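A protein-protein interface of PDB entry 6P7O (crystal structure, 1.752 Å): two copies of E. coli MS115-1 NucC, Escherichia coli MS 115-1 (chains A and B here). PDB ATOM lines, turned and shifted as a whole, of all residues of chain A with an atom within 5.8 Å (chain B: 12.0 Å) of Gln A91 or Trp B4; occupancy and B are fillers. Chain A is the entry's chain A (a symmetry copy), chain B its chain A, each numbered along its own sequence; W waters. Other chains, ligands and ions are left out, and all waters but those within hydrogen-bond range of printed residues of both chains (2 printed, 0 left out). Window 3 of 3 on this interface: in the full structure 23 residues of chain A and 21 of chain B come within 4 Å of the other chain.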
ATOM      1  N   ASN A  58       3.462  -4.742  17.916  1.00  0.00           N
ATOM      2  CA  ASN A  58       4.720  -5.032  18.599  1.00  0.00           C
ATOM      3  C   ASN A  58       5.659  -5.701  17.597  1.00  0.00           C
ATOM      4  O   ASN A  58       5.269  -6.690  17.000  1.00  0.00           O
ATOM      5  CB  ASN A  58       4.377  -5.952  19.759  1.00  0.00           C
ATOM      6  CG  ASN A  58       5.626  -6.464  20.570  1.00  0.00           C
ATOM      7  OD1 ASN A  58       5.605  -7.603  21.040  1.00  0.00           O
ATOM      8  ND2 ASN A  58       6.570  -5.646  20.797  1.00  0.00           N
ATOM      9  N   PHE A  60       9.893  -6.138  15.694  1.00  0.00           N
ATOM     10  CA  PHE A  60      11.252  -5.736  15.348  1.00  0.00           C
ATOM     11  C   PHE A  60      11.281  -4.986  14.019  1.00  0.00           C
ATOM     12  O   PHE A  60      10.420  -5.153  13.179  1.00  0.00           O
ATOM     13  CB  PHE A  60      12.217  -6.940  15.235  1.00  0.00           C
ATOM     14  CG  PHE A  60      12.395  -7.706  16.516  1.00  0.00           C
ATOM     15  CD1 PHE A  60      11.447  -8.663  16.950  1.00  0.00           C
ATOM     16  CD2 PHE A  60      13.556  -7.520  17.261  1.00  0.00           C
ATOM     17  CE1 PHE A  60      11.621  -9.359  18.103  1.00  0.00           C
ATOM     18  CE2 PHE A  60      13.750  -8.207  18.481  1.00  0.00           C
ATOM     19  CZ  PHE A  60      12.759  -9.163  18.895  1.00  0.00           C
ATOM     20  N   PHE A  68      19.110  -5.498  12.947  1.00  0.00           N
ATOM     21  CA  PHE A  68      17.795  -5.481  13.575  1.00  0.00           C
ATOM     22  C   PHE A  68      17.798  -4.420  14.650  1.00  0.00           C
ATOM     23  O   PHE A  68      18.795  -4.245  15.347  1.00  0.00           O
ATOM     24  CB  PHE A  68      17.445  -6.834  14.218  1.00  0.00           C
ATOM     25  CG  PHE A  68      17.165  -7.948  13.228  1.00  0.00           C
ATOM     26  CD1 PHE A  68      18.187  -8.708  12.690  1.00  0.00           C
ATOM     27  CD2 PHE A  68      15.854  -8.296  12.914  1.00  0.00           C
ATOM     28  CE1 PHE A  68      17.913  -9.736  11.845  1.00  0.00           C
ATOM     29  CE2 PHE A  68      15.585  -9.347  12.083  1.00  0.00           C
ATOM     30  CZ  PHE A  68      16.626 -10.070  11.559  1.00  0.00           C
ATOM     31  N   GLN A  71      13.550  -5.075  20.173  1.00  0.00           N
ATOM     32  CA  GLN A  71      12.116  -5.285  20.041  1.00  0.00           C
ATOM     33  C   GLN A  71      11.379  -4.017  20.460  1.00  0.00           C
ATOM     34  O   GLN A  71      11.625  -3.484  21.557  1.00  0.00           O
ATOM     35  CB  GLN A  71      11.672  -6.437  20.914  1.00  0.00           C
ATOM     36  CG  GLN A  71      10.222  -6.830  20.605  1.00  0.00           C
ATOM     37  CD  GLN A  71       9.770  -7.995  21.476  1.00  0.00           C
ATOM     38  OE1 GLN A  71      10.579  -8.571  22.204  1.00  0.00           O
ATOM     39  NE2 GLN A  71       8.491  -8.325  21.420  1.00  0.00           N
ATOM     40  N   PHE A  86       7.503  -9.639   7.886  1.00  0.00           N
ATOM     41  CA  PHE A  86       7.861 -11.014   8.236  1.00  0.00           C
ATOM     42  C   PHE A  86       7.091 -11.430   9.483  1.00  0.00           C
ATOM     43  O   PHE A  86       6.990 -10.624  10.437  1.00  0.00           O
ATOM     44  CB  PHE A  86       9.375 -11.178   8.505  1.00  0.00           C
ATOM     45  CG  PHE A  86      10.241 -11.052   7.262  1.00  0.00           C
ATOM     46  CD1 PHE A  86      10.204 -11.981   6.293  1.00  0.00           C
ATOM     47  CD2 PHE A  86      11.092  -9.993   7.151  1.00  0.00           C
ATOM     48  CE1 PHE A  86      11.004 -11.867   5.167  1.00  0.00           C
ATOM     49  CE2 PHE A  86      11.841  -9.816   6.048  1.00  0.00           C
ATOM     50  CZ  PHE A  86      11.828 -10.773   5.073  1.00  0.00           C
ATOM     51  N   LYS A  87       6.676 -12.717   9.525  1.00  0.00           N
ATOM     52  CA  LYS A  87       6.044 -13.340  10.700  1.00  0.00           C
ATOM     53  C   LYS A  87       6.916 -14.534  11.045  1.00  0.00           C
ATOM     54  O   LYS A  87       7.037 -15.480  10.250  1.00  0.00           O
ATOM     55  CB  LYS A  87       4.608 -13.785  10.473  1.00  0.00           C
ATOM     56  CG  LYS A  87       3.750 -12.779   9.750  1.00  0.00           C
ATOM     57  CD  LYS A  87       3.450 -11.584  10.588  1.00  0.00           C
ATOM     58  CE  LYS A  87       2.670 -10.528   9.780  1.00  0.00           C
ATOM     59  NZ  LYS A  87       1.360 -11.000   9.216  1.00  0.00           N
ATOM     60  N   PHE A  88       7.633 -14.445  12.154  1.00  0.00           N
ATOM     61  CA  PHE A  88       8.658 -15.430  12.471  1.00  0.00           C
ATOM     62  C   PHE A  88       8.637 -15.751  13.952  1.00  0.00           C
ATOM     63  O   PHE A  88       8.763 -14.833  14.763  1.00  0.00           O
ATOM     64  CB  PHE A  88      10.025 -14.862  12.077  1.00  0.00           C
ATOM     65  CG  PHE A  88      11.152 -15.801  12.291  1.00  0.00           C
ATOM     66  CD1 PHE A  88      11.315 -16.946  11.491  1.00  0.00           C
ATOM     67  CD2 PHE A  88      12.056 -15.556  13.303  1.00  0.00           C
ATOM     68  CE1 PHE A  88      12.394 -17.836  11.719  1.00  0.00           C
ATOM     69  CE2 PHE A  88      13.102 -16.400  13.540  1.00  0.00           C
ATOM     70  CZ  PHE A  88      13.294 -17.567  12.717  1.00  0.00           C
ATOM     71  N   ASN A  89       8.467 -17.017  14.310  1.00  0.00           N
ATOM     72  CA  ASN A  89       8.559 -17.425  15.726  1.00  0.00           C
ATOM     73  C   ASN A  89       7.665 -16.550  16.601  1.00  0.00           C
ATOM     74  O   ASN A  89       8.070 -16.051  17.666  1.00  0.00           O
ATOM     75  CB  ASN A  89      10.012 -17.372  16.222  1.00  0.00           C
ATOM     76  CG  ASN A  89      10.890 -18.498  15.617  1.00  0.00           C
ATOM     77  OD1 ASN A  89      10.419 -19.330  14.819  1.00  0.00           O
ATOM     78  ND2 ASN A  89      12.168 -18.511  15.996  1.00  0.00           N
ATOM     79  N   GLU A  90       6.456 -16.295  16.092  1.00  0.00           N
ATOM     80  CA  GLU A  90       5.437 -15.540  16.775  1.00  0.00           C
ATOM     81  C   GLU A  90       5.815 -14.077  16.974  1.00  0.00           C
ATOM     82  O   GLU A  90       5.176 -13.394  17.750  1.00  0.00           O
ATOM     83  CB  GLU A  90       5.097 -16.207  18.116  1.00  0.00           C
ATOM     84  CG  GLU A  90       4.447 -17.590  17.890  1.00  0.00           C
ATOM     85  CD  GLU A  90       4.123 -18.307  19.176  1.00  0.00           C
ATOM     86  OE1 GLU A  90       4.765 -17.998  20.208  1.00  0.00           O
ATOM     87  OE2 GLU A  90       3.225 -19.178  19.142  1.00  0.00           O
ATOM     88  N   GLN A  91       6.793 -13.545  16.247  1.00  0.00           N
ATOM     89  CA  GLN A  91       7.135 -12.130  16.258  1.00  0.00           C
ATOM     90  C   GLN A  91       6.853 -11.533  14.876  1.00  0.00           C
ATOM     91  O   GLN A  91       6.661 -12.244  13.879  1.00  0.00           O
ATOM     92  CB  GLN A  91       8.604 -11.909  16.596  1.00  0.00           C
ATOM     93  CG  GLN A  91       9.125 -12.709  17.796  1.00  0.00           C
ATOM     94  CD  GLN A  91       8.675 -12.056  19.071  1.00  0.00           C
ATOM     95  OE1 GLN A  91       8.201 -10.887  19.085  1.00  0.00           O
ATOM     96  NE2 GLN A  91       8.802 -12.790  20.152  1.00  0.00           N
ATOM     97  N   ILE A  92       6.825 -10.227  14.835  1.00  0.00           N
ATOM     98  CA  ILE A  92       6.579  -9.478  13.611  1.00  0.00           C
ATOM     99  C   ILE A  92       7.828  -8.663  13.330  1.00  0.00           C
ATOM    100  O   ILE A  92       8.435  -8.100  14.255  1.00  0.00           O
ATOM    101  CB  ILE A  92       5.353  -8.548  13.763  1.00  0.00           C
ATOM    102  CG1 ILE A  92       4.111  -9.405  14.056  1.00  0.00           C
ATOM    103  CG2 ILE A  92       5.239  -7.600  12.562  1.00  0.00           C
ATOM    104  CD1 ILE A  92       2.926  -8.504  14.376  1.00  0.00           C
ATOM    105  N   ILE A  93       8.255  -8.619  12.049  1.00  0.00           N
ATOM    106  CA  ILE A  93       9.429  -7.856  11.666  1.00  0.00           C
ATOM    107  C   ILE A  93       9.113  -7.015  10.436  1.00  0.00           C
ATOM    108  O   ILE A  93       8.655  -7.549   9.430  1.00  0.00           O
ATOM    109  CB  ILE A  93      10.638  -8.765  11.384  1.00  0.00           C
ATOM    110  CG1 ILE A  93      10.937  -9.696  12.578  1.00  0.00           C
ATOM    111  CG2 ILE A  93      11.894  -7.874  11.131  1.00  0.00           C
ATOM    112  CD1 ILE A  93      10.355 -11.116  12.468  1.00  0.00           C
ATOM    113  N   TRP B   4      19.399 -15.054  15.352  1.00  0.00           N
ATOM    114  CA  TRP B   4      18.481 -14.523  14.321  1.00  0.00           C
ATOM    115  C   TRP B   4      19.145 -13.815  13.153  1.00  0.00           C
ATOM    116  O   TRP B   4      20.046 -12.993  13.363  1.00  0.00           O
ATOM    117  CB  TRP B   4      17.535 -13.484  14.905  1.00  0.00           C
ATOM    118  CG  TRP B   4      16.302 -13.932  15.527  1.00  0.00           C
ATOM    119  CD1 TRP B   4      16.081 -15.068  16.274  1.00  0.00           C
ATOM    120  CD2 TRP B   4      15.075 -13.224  15.491  1.00  0.00           C
ATOM    121  NE1 TRP B   4      14.774 -15.099  16.699  1.00  0.00           N
ATOM    122  CE2 TRP B   4      14.134 -13.970  16.237  1.00  0.00           C
ATOM    123  CE3 TRP B   4      14.673 -12.010  14.920  1.00  0.00           C
ATOM    124  CZ2 TRP B   4      12.802 -13.537  16.409  1.00  0.00           C
ATOM    125  CZ3 TRP B   4      13.358 -11.598  15.086  1.00  0.00           C
ATOM    126  CH2 TRP B   4      12.440 -12.361  15.810  1.00  0.00           C
ATOM    127  N   SER B   5      18.683 -14.076  11.927  1.00  0.00           N
ATOM    128  CA  SER B   5      19.293 -13.430  10.781  1.00  0.00           C
ATOM    129  C   SER B   5      18.229 -13.182   9.718  1.00  0.00           C
ATOM    130  O   SER B   5      17.171 -13.825   9.677  1.00  0.00           O
ATOM    131  CB  SER B   5      20.446 -14.265  10.199  1.00  0.00           C
ATOM    132  OG  SER B   5      19.913 -15.288   9.363  1.00  0.00           O
ATOM    133  N   LEU B   6      18.492 -12.202   8.863  1.00  0.00           N
ATOM    134  CA  LEU B   6      17.534 -11.908   7.823  1.00  0.00           C
ATOM    135  C   LEU B   6      17.410 -13.080   6.867  1.00  0.00           C
ATOM    136  O   LEU B   6      16.336 -13.350   6.326  1.00  0.00           O
ATOM    137  CB  LEU B   6      17.942 -10.629   7.129  1.00  0.00           C
ATOM    138  CG  LEU B   6      17.085 -10.129   6.013  1.00  0.00           C
ATOM    139  CD1 LEU B   6      15.569  -9.973   6.419  1.00  0.00           C
ATOM    140  CD2 LEU B   6      17.627  -8.791   5.575  1.00  0.00           C
ATOM    141  N   SER B   7      18.489 -13.842   6.703  1.00  0.00           N
ATOM    142  CA  SER B   7      18.395 -15.032   5.860  1.00  0.00           C
ATOM    143  C   SER B   7      17.371 -16.020   6.406  1.00  0.00           C
ATOM    144  O   SER B   7      16.675 -16.660   5.619  1.00  0.00           O
ATOM    145  CB  SER B   7      19.775 -15.722   5.773  1.00  0.00           C
ATOM    146  OG  SER B   7      20.731 -14.843   5.264  1.00  0.00           O
ATOM    147  N   GLN B   8      17.355 -16.230   7.739  1.00  0.00           N
ATOM    148  CA  GLN B   8      16.423 -17.156   8.370  1.00  0.00           C
ATOM    149  C   GLN B   8      14.987 -16.674   8.203  1.00  0.00           C
ATOM    150  O   GLN B   8      14.062 -17.474   8.017  1.00  0.00           O
ATOM    151  CB  GLN B   8      16.732 -17.310   9.879  1.00  0.00           C
ATOM    152  CG  GLN B   8      18.014 -18.005  10.209  1.00  0.00           C
ATOM    153  CD  GLN B   8      18.505 -17.724  11.673  1.00  0.00           C
ATOM    154  OE1 GLN B   8      17.707 -17.499  12.596  1.00  0.00           O
ATOM    155  NE2 GLN B   8      19.823 -17.739  11.855  1.00  0.00           N
ATOM    156  N   LEU B   9      14.750 -15.367   8.328  1.00  0.00           N
ATOM    157  CA  LEU B   9      13.408 -14.881   8.038  1.00  0.00           C
ATOM    158  C   LEU B   9      12.960 -15.249   6.642  1.00  0.00           C
ATOM    159  O   LEU B   9      11.778 -15.562   6.420  1.00  0.00           O
ATOM    160  CB  LEU B   9      13.351 -13.364   8.275  1.00  0.00           C
ATOM    161  CG  LEU B   9      13.107 -12.870   9.717  1.00  0.00           C
ATOM    162  CD1 LEU B   9      13.809 -13.530  10.765  1.00  0.00           C
ATOM    163  CD2 LEU B   9      13.388 -11.333   9.791  1.00  0.00           C
ATOM    164  N   PHE B  10      13.841 -15.081   5.643  1.00  0.00           N
ATOM    165  CA  PHE B  10      13.443 -15.401   4.277  1.00  0.00           C
ATOM    166  C   PHE B  10      13.196 -16.920   4.120  1.00  0.00           C
ATOM    167  O   PHE B  10      12.285 -17.351   3.382  1.00  0.00           O
ATOM    168  CB  PHE B  10      14.542 -14.932   3.279  1.00  0.00           C
ATOM    169  CG  PHE B  10      14.366 -13.492   2.792  1.00  0.00           C
ATOM    170  CD1 PHE B  10      13.365 -13.210   1.872  1.00  0.00           C
ATOM    171  CD2 PHE B  10      15.219 -12.494   3.218  1.00  0.00           C
ATOM    172  CE1 PHE B  10      13.166 -11.945   1.406  1.00  0.00           C
ATOM    173  CE2 PHE B  10      15.020 -11.165   2.759  1.00  0.00           C
ATOM    174  CZ  PHE B  10      13.997 -10.928   1.830  1.00  0.00           C
ATOM    175  N   ALA B  11      14.040 -17.727   4.769  1.00  0.00           N
ATOM    176  CA  ALA B  11      13.860 -19.182   4.697  1.00  0.00           C
ATOM    177  C   ALA B  11      12.531 -19.553   5.320  1.00  0.00           C
ATOM    178  O   ALA B  11      11.814 -20.372   4.783  1.00  0.00           O
ATOM    179  CB  ALA B  11      15.013 -19.927   5.419  1.00  0.00           C
ATOM    180  N   SER B  12      12.148 -18.922   6.434  1.00  0.00           N
ATOM    181  CA  SER B  12      10.877 -19.272   7.059  1.00  0.00           C
ATOM    182  C   SER B  12       9.693 -18.750   6.270  1.00  0.00           C
ATOM    183  O   SER B  12       8.688 -19.458   6.134  1.00  0.00           O
ATOM    184  CB  SER B  12      10.859 -18.785   8.524  1.00  0.00           C
ATOM    185  OG  SER B  12       9.624 -19.085   9.144  1.00  0.00           O
ATOM    186  N   LEU B  13       9.821 -17.582   5.632  1.00  0.00           N
ATOM    187  CA  LEU B  13       8.773 -17.159   4.724  1.00  0.00           C
ATOM    188  C   LEU B  13       8.604 -18.149   3.569  1.00  0.00           C
ATOM    189  O   LEU B  13       7.466 -18.454   3.178  1.00  0.00           O
ATOM    190  CB  LEU B  13       9.048 -15.750   4.197  1.00  0.00           C
ATOM    191  CG  LEU B  13       8.224 -15.245   3.000  1.00  0.00           C
ATOM    192  CD1 LEU B  13       6.748 -15.089   3.385  1.00  0.00           C
ATOM    193  CD2 LEU B  13       8.824 -13.890   2.566  1.00  0.00           C
ATOM    194  N   ASP B  16       6.670 -21.147   4.580  1.00  0.00           N
ATOM    195  CA  ASP B  16       5.251 -20.883   4.673  1.00  0.00           C
ATOM    196  C   ASP B  16       4.625 -20.815   3.292  1.00  0.00           C
ATOM    197  O   ASP B  16       3.521 -21.294   3.084  1.00  0.00           O
ATOM    198  CB  ASP B  16       5.023 -19.562   5.390  1.00  0.00           C
ATOM    199  CG  ASP B  16       5.515 -19.561   6.865  1.00  0.00           C
ATOM    200  OD1 ASP B  16       5.769 -20.653   7.457  1.00  0.00           O
ATOM    201  OD2 ASP B  16       5.664 -18.431   7.386  1.00  0.00           O
ATOM    202  N   TYR B  49       0.474 -12.180   0.288  1.00  0.00           N
ATOM    203  CA  TYR B  49       1.786 -11.585   0.501  1.00  0.00           C
ATOM    204  C   TYR B  49       2.068 -10.349  -0.339  1.00  0.00           C
ATOM    205  O   TYR B  49       3.035  -9.672  -0.046  1.00  0.00           O
ATOM    206  CB  TYR B  49       2.911 -12.631   0.214  1.00  0.00           C
ATOM    207  CG  TYR B  49       2.974 -13.672   1.302  1.00  0.00           C
ATOM    208  CD1 TYR B  49       3.499 -13.370   2.510  1.00  0.00           C
ATOM    209  CD2 TYR B  49       2.476 -14.942   1.107  1.00  0.00           C
ATOM    210  CE1 TYR B  49       3.545 -14.270   3.558  1.00  0.00           C
ATOM    211  CE2 TYR B  49       2.526 -15.875   2.134  1.00  0.00           C
ATOM    212  CZ  TYR B  49       3.060 -15.537   3.358  1.00  0.00           C
ATOM    213  OH  TYR B  49       3.148 -16.442   4.440  1.00  0.00           O
HETATM  214  O   HOH W   1       9.517 -14.906   7.987  1.00  0.00           O
HETATM  215  O   HOH W   2       7.778 -17.366   8.748  1.00  0.00           O
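Among the printed residues, pairs that only touch across the chains: Phe A60 with Trp B4 (3.9 Å), Phe A68 with Trp B4 (3.996 Å), Phe A68 with Ser B5 (3.96 Å), Phe A68 with Leu B6 (3.9 Å), Phe A68 with Leu B9 (3.7 Å), Phe A86 with Leu B6 (3.7 Å), Phe A86 with Leu B9 (3.7 Å), Phe A86 with Phe B10 (3.9 Å), Phe A86 with Leu B13 (3.95 Å), Phe A88 with Trp B4 (3.8 Å), Phe A88 with Leu B9 (3.7 Å), Phe A88 with Ser B12 (3.5 Å), Gln A91 with Trp B4 (3.9 Å), Ile A93 with Trp B4 (3.97 Å) and Ile A93 with Leu B9 (3.999 Å).
Printed residues of chain B that touch a printed residue of chain A: Trp B4, Ser B5, Leu B6, Leu B9, Phe B10, Ser B12 and Leu B13.
Hydrophobic or aromatic side chains of chain B within 4 Å of the printed part of chain A: Trp B4, Leu B6, Leu B9, Phe B10 and Leu B13.
Among the printed residues, no Asp or Glu carboxylate lies within 4 Å of a Lys or Arg side-chain nitrogen of the other chain.
Water W2 lies within hydrogen-bond range of the backbone carbonyl oxygen (O) of Lys A87 (2.5 Å), the side-chain hydroxyl (OG) of Ser B12 (2.6 Å) and the side-chain carboxylate (OD2) of Asp B16 (2.7 Å).
Water W1 lies within hydrogen-bond range of the backbone carbonyl oxygen (O) of Leu B9 (2.8 Å) and the backbone carbonyl oxygen (O) of Lys A87 (3.4 Å).
Of the printed residues of chain B, Gln A91 touches Trp B4.
Printed residues of chain A within 4 Å of Trp B4: Phe A60, Phe A68, Phe A88, Gln A91 and Ile A93.
No residue of chain B comes within 4 Å of Asn A58.
Phe A60 touches one residue of chain B.
Phe A88 touches just these residues of chain B: Trp B4, Leu B9 and Ser B12.
Asn A89 touches none of the printed residues of chain B.
Of the printed residues of chain A, Ser B12 touches Phe A88 (3.5 Å).
Printed residues of chain A within 4 Å of Ser B5: Phe A68.
Of the printed residues of chain A, Leu B6 touches Phe A68 and Phe A86.
Printed residues of chain A within 4 Å of Leu B9: Phe A68 (3.7 Å), Phe A86 (3.7 Å), Phe A88 (3.7 Å) and Ile A93 (3.999 Å).
Printed residues of chain B within 4 Å of Ile A93: Trp B4 and Leu B9.
Gln A71 touches none of the printed residues of chain B.
The nearest printed residue of chain A that does not touch Trp B4 is Asn A89 (4.4 Å).
No position is printed for both chains.
The side-chain hydroxyl of Ser B5 sits at hydrogen-bond distance from the backbone NH of Gln B8, at 3.2 Å.
The backbone NH (N) of Phe A60 sits at hydrogen-bond distance from the backbone carbonyl oxygen (O) of Ile A92 (2.8 Å).
OE1 of Gln A91 lies within hydrogen-bond range of NE2 of Gln A71 (3.5 Å).
N of Phe A86 lies within hydrogen-bond range of O of Ile A93 (2.8 Å).
The backbone NH (N) of Ser B7 sits close to the side-chain hydroxyl (OG) of Ser B5 (3.3 Å).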
